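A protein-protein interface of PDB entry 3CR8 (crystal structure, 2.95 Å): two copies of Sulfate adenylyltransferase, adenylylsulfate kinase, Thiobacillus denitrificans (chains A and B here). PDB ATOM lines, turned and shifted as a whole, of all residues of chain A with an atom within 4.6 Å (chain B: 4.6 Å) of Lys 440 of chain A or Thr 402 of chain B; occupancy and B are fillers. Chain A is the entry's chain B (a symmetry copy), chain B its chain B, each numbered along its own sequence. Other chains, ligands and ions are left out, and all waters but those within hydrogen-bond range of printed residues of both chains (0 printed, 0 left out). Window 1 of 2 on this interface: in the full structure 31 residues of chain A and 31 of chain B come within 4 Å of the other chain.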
ATOM      1  N   SER A 436      27.087 -14.543  -8.048  1.00  0.00           N
ATOM      2  CA  SER A 436      27.507 -15.327  -6.872  1.00  0.00           C
ATOM      3  C   SER A 436      26.732 -14.975  -5.604  1.00  0.00           C
ATOM      4  O   SER A 436      26.403 -15.849  -4.817  1.00  0.00           O
ATOM      5  CB  SER A 436      29.016 -15.184  -6.603  1.00  0.00           C
ATOM      6  OG  SER A 436      29.357 -13.868  -6.161  1.00  0.00           O
ATOM      7  N   GLU A 437      26.456 -13.693  -5.396  1.00  0.00           N
ATOM      8  CA  GLU A 437      25.597 -13.285  -4.290  1.00  0.00           C
ATOM      9  C   GLU A 437      24.181 -13.888  -4.394  1.00  0.00           C
ATOM     10  O   GLU A 437      23.681 -14.419  -3.413  1.00  0.00           O
ATOM     11  CB  GLU A 437      25.536 -11.759  -4.168  1.00  0.00           C
ATOM     12  CG  GLU A 437      26.820 -11.144  -3.734  1.00  0.00           C
ATOM     13  CD  GLU A 437      27.108 -11.290  -2.252  1.00  0.00           C
ATOM     14  OE1 GLU A 437      26.225 -10.916  -1.447  1.00  0.00           O
ATOM     15  OE2 GLU A 437      28.237 -11.736  -1.900  1.00  0.00           O
ATOM     16  N   ILE A 438      23.552 -13.811  -5.566  1.00  0.00           N
ATOM     17  CA  ILE A 438      22.286 -14.486  -5.775  1.00  0.00           C
ATOM     18  C   ILE A 438      22.367 -15.971  -5.357  1.00  0.00           C
ATOM     19  O   ILE A 438      21.431 -16.497  -4.719  1.00  0.00           O
ATOM     20  CB  ILE A 438      21.745 -14.398  -7.242  1.00  0.00           C
ATOM     21  CG1 ILE A 438      21.681 -12.953  -7.737  1.00  0.00           C
ATOM     22  CG2 ILE A 438      20.335 -14.975  -7.322  1.00  0.00           C
ATOM     23  CD1 ILE A 438      20.997 -12.025  -6.773  1.00  0.00           C
ATOM     24  N   THR A 439      23.466 -16.649  -5.694  1.00  0.00           N
ATOM     25  CA  THR A 439      23.493 -18.091  -5.517  1.00  0.00           C
ATOM     26  C   THR A 439      23.858 -18.504  -4.101  1.00  0.00           C
ATOM     27  O   THR A 439      23.201 -19.395  -3.510  1.00  0.00           O
ATOM     28  CB  THR A 439      24.282 -18.844  -6.630  1.00  0.00           C
ATOM     29  OG1 THR A 439      25.254 -19.726  -6.043  1.00  0.00           O
ATOM     30  CG2 THR A 439      24.949 -17.892  -7.532  1.00  0.00           C
ATOM     31  N   LYS A 440      24.892 -17.857  -3.565  1.00  0.00           N
ATOM     32  CA  LYS A 440      25.225 -17.932  -2.140  1.00  0.00           C
ATOM     33  C   LYS A 440      23.958 -17.884  -1.280  1.00  0.00           C
ATOM     34  O   LYS A 440      23.832 -18.646  -0.343  1.00  0.00           O
ATOM     35  CB  LYS A 440      26.136 -16.757  -1.789  1.00  0.00           C
ATOM     36  CG  LYS A 440      26.360 -16.457  -0.310  1.00  0.00           C
ATOM     37  CD  LYS A 440      26.672 -14.969  -0.163  1.00  0.00           C
ATOM     38  CE  LYS A 440      27.476 -14.643   1.090  1.00  0.00           C
ATOM     39  NZ  LYS A 440      28.105 -13.286   0.923  1.00  0.00           N
ATOM     40  N   ASN A 441      23.028 -16.990  -1.624  1.00  0.00           N
ATOM     41  CA  ASN A 441      21.783 -16.830  -0.896  1.00  0.00           C
ATOM     42  C   ASN A 441      20.627 -17.749  -1.311  1.00  0.00           C
ATOM     43  O   ASN A 441      19.468 -17.484  -0.955  1.00  0.00           O
ATOM     44  CB  ASN A 441      21.333 -15.380  -0.991  1.00  0.00           C
ATOM     45  CG  ASN A 441      21.579 -14.613   0.294  1.00  0.00           C
ATOM     46  OD1 ASN A 441      21.054 -14.973   1.376  1.00  0.00           O
ATOM     47  ND2 ASN A 441      22.372 -13.539   0.189  1.00  0.00           N
ATOM     48  N   ARG A 442      20.929 -18.810  -2.061  1.00  0.00           N
ATOM     49  CA  ARG A 442      19.925 -19.809  -2.423  1.00  0.00           C
ATOM     50  C   ARG A 442      19.008 -19.422  -3.582  1.00  0.00           C
ATOM     51  O   ARG A 442      17.907 -19.933  -3.667  1.00  0.00           O
ATOM     52  CB  ARG A 442      19.068 -20.142  -1.196  1.00  0.00           C
ATOM     53  CG  ARG A 442      19.298 -21.531  -0.569  1.00  0.00           C
ATOM     54  CD  ARG A 442      20.698 -22.091  -0.845  1.00  0.00           C
ATOM     55  NE  ARG A 442      21.762 -21.845   0.152  1.00  0.00           N
ATOM     56  CZ  ARG A 442      21.630 -21.292   1.363  1.00  0.00           C
ATOM     57  NH1 ARG A 442      20.445 -20.877   1.817  1.00  0.00           N
ATOM     58  NH2 ARG A 442      22.720 -21.151   2.125  1.00  0.00           N
ATOM     59  N   VAL A 467      30.256 -21.097  -3.718  1.00  0.00           N
ATOM     60  CA  VAL A 467      29.183 -20.626  -2.883  1.00  0.00           C
ATOM     61  C   VAL A 467      27.890 -21.356  -3.291  1.00  0.00           C
ATOM     62  O   VAL A 467      26.844 -21.238  -2.640  1.00  0.00           O
ATOM     63  CB  VAL A 467      29.114 -19.063  -3.001  1.00  0.00           C
ATOM     64  CG1 VAL A 467      28.114 -18.617  -4.069  1.00  0.00           C
ATOM     65  CG2 VAL A 467      28.822 -18.425  -1.656  1.00  0.00           C
ATOM     66  N   CYS B 400      22.048 -15.557   5.241  1.00  0.00           N
ATOM     67  CA  CYS B 400      23.456 -15.234   4.991  1.00  0.00           C
ATOM     68  C   CYS B 400      23.702 -13.728   5.020  1.00  0.00           C
ATOM     69  O   CYS B 400      22.877 -12.956   4.556  1.00  0.00           O
ATOM     70  CB  CYS B 400      23.954 -15.846   3.677  1.00  0.00           C
ATOM     71  SG  CYS B 400      24.035 -17.648   3.735  1.00  0.00           S
ATOM     72  N   VAL B 401      24.825 -13.308   5.601  1.00  0.00           N
ATOM     73  CA  VAL B 401      25.147 -11.886   5.690  1.00  0.00           C
ATOM     74  C   VAL B 401      26.283 -11.521   4.733  1.00  0.00           C
ATOM     75  O   VAL B 401      27.301 -12.205   4.665  1.00  0.00           O
ATOM     76  CB  VAL B 401      25.547 -11.470   7.108  1.00  0.00           C
ATOM     77  CG1 VAL B 401      25.841  -9.974   7.141  1.00  0.00           C
ATOM     78  CG2 VAL B 401      24.463 -11.859   8.105  1.00  0.00           C
ATOM     79  N   THR B 402      26.093 -10.442   3.987  1.00  0.00           N
ATOM     80  CA  THR B 402      27.135  -9.921   3.110  1.00  0.00           C
ATOM     81  C   THR B 402      27.472  -8.462   3.432  1.00  0.00           C
ATOM     82  O   THR B 402      26.593  -7.610   3.495  1.00  0.00           O
ATOM     83  CB  THR B 402      26.725  -9.979   1.645  1.00  0.00           C
ATOM     84  OG1 THR B 402      26.636 -11.344   1.222  1.00  0.00           O
ATOM     85  CG2 THR B 402      27.764  -9.251   0.811  1.00  0.00           C
ATOM     86  N   LEU B 403      28.750  -8.185   3.647  1.00  0.00           N
ATOM     87  CA  LEU B 403      29.186  -6.846   3.957  1.00  0.00           C
ATOM     88  C   LEU B 403      29.596  -6.195   2.657  1.00  0.00           C
ATOM     89  O   LEU B 403      30.670  -6.488   2.120  1.00  0.00           O
ATOM     90  CB  LEU B 403      30.403  -6.901   4.883  1.00  0.00           C
ATOM     91  CG  LEU B 403      30.500  -5.825   5.965  1.00  0.00           C
ATOM     92  CD1 LEU B 403      31.868  -5.840   6.586  1.00  0.00           C
ATOM     93  CD2 LEU B 403      30.173  -4.447   5.423  1.00  0.00           C
ATOM     94  N   LEU B 404      28.752  -5.317   2.135  1.00  0.00           N
ATOM     95  CA  LEU B 404      29.105  -4.519   0.955  1.00  0.00           C
ATOM     96  C   LEU B 404      29.839  -3.220   1.340  1.00  0.00           C
ATOM     97  O   LEU B 404      29.232  -2.138   1.384  1.00  0.00           O
ATOM     98  CB  LEU B 404      27.840  -4.174   0.175  1.00  0.00           C
ATOM     99  CG  LEU B 404      27.193  -5.332  -0.581  1.00  0.00           C
ATOM    100  CD1 LEU B 404      25.889  -4.876  -1.253  1.00  0.00           C
ATOM    101  CD2 LEU B 404      28.178  -5.908  -1.599  1.00  0.00           C
ATOM    102  N   ILE B 444      20.743 -11.008   4.279  1.00  0.00           N
ATOM    103  CA  ILE B 444      20.807  -9.663   4.823  1.00  0.00           C
ATOM    104  C   ILE B 444      22.027  -8.959   4.252  1.00  0.00           C
ATOM    105  O   ILE B 444      23.128  -9.500   4.306  1.00  0.00           O
ATOM    106  CB  ILE B 444      20.733  -9.576   6.384  1.00  0.00           C
ATOM    107  CG1 ILE B 444      22.085  -9.314   6.992  1.00  0.00           C
ATOM    108  CG2 ILE B 444      20.123 -10.801   7.034  1.00  0.00           C
ATOM    109  CD1 ILE B 444      22.025  -9.414   8.478  1.00  0.00           C
ATOM    110  N   ALA B 445      21.820  -7.770   3.676  1.00  0.00           N
ATOM    111  CA  ALA B 445      22.911  -6.982   3.100  1.00  0.00           C
ATOM    112  C   ALA B 445      23.240  -5.714   3.906  1.00  0.00           C
ATOM    113  O   ALA B 445      22.353  -4.930   4.216  1.00  0.00           O
ATOM    114  CB  ALA B 445      22.580  -6.630   1.684  1.00  0.00           C
ATOM    115  N   ILE B 446      24.512  -5.507   4.234  1.00  0.00           N
ATOM    116  CA  ILE B 446      24.896  -4.386   5.078  1.00  0.00           C
ATOM    117  C   ILE B 446      25.796  -3.440   4.322  1.00  0.00           C
ATOM    118  O   ILE B 446      26.927  -3.789   3.964  1.00  0.00           O
ATOM    119  CB  ILE B 446      25.661  -4.865   6.321  1.00  0.00           C
ATOM    120  CG1 ILE B 446      24.749  -5.716   7.207  1.00  0.00           C
ATOM    121  CG2 ILE B 446      26.293  -3.677   7.072  1.00  0.00           C
ATOM    122  CD1 ILE B 446      25.543  -6.621   8.116  1.00  0.00           C
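Of the 8 printed residues of chain A, 3 touch a printed residue of chain B.
Printed residues of chain A that touch a printed residue of chain B: Glu 437, Lys 440 and Asn 441.
Of the 8 printed residues of chain B, 3 touch a printed residue of chain A.
Among the printed residues, no Asp or Glu carboxylate lies within 4 Å of a Lys or Arg side-chain nitrogen of the other chain.
Of chain B, only Val 401 (3.98 Å) and Thr 402 (2.5 Å) come within 4 Å of Lys 440 of chain A.
Thr 402 of chain B touches just these residues of chain A: Glu 437 (2.7 Å) and Lys 440 (2.5 Å).
Of the printed residues of chain B, Asn 441 of chain A touches Cys 400.
Of the printed residues of chain B, Glu 437 of chain A touches Thr 402 (2.7 Å).
Of the printed residues of chain A, Val 401 of chain B touches Lys 440.
Of the printed residues of chain A, Cys 400 of chain B touches Asn 441 (3.8 Å).
Ile 438 of chain A touches none of the printed residues of chain B.
The nearest residue of chain B that does not touch Lys 440 of chain A is Cys 400 of chain B (4.2 Å).
No position is printed for both chains.
Of the 4 pairs that touch across the chains among the printed residues, none has its exchanged pair printed and touching as well.
OG1 of Thr 402 of chain B sits at hydrogen-bond distance from OE1 of Glu 437 of chain A (2.7 Å).
The side-chain amino group of Lys 440 of chain A sits at hydrogen-bond distance from the side-chain hydroxyl of Thr 402 of chain B.
Among the printed residues, merely in contact across the chains: Lys 440 of chain A with Val 401 of chain B (3.98 Å) and Asn 441 of chain A with Cys 400 of chain B (3.8 Å).
The backbone carbonyl oxygen of Cys 400 of chain B lies within hydrogen-bond range of the backbone NH of Ile 444 of chain B, at 2.9 Å.
N of Thr 402 of chain B lies within hydrogen-bond range of O of Ile 444 of chain B, at 3.1 Å.
The backbone NH of Ile 446 of chain B is in hydrogen-bond range of the backbone carbonyl oxygen of Thr 402 of chain B (3.0 Å).
The side-chain carboxylate (OE2) of Glu 437 of chain A is in salt-bridge range of the side-chain amino group (NZ) of Lys 440 of chain A (3.2 Å).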
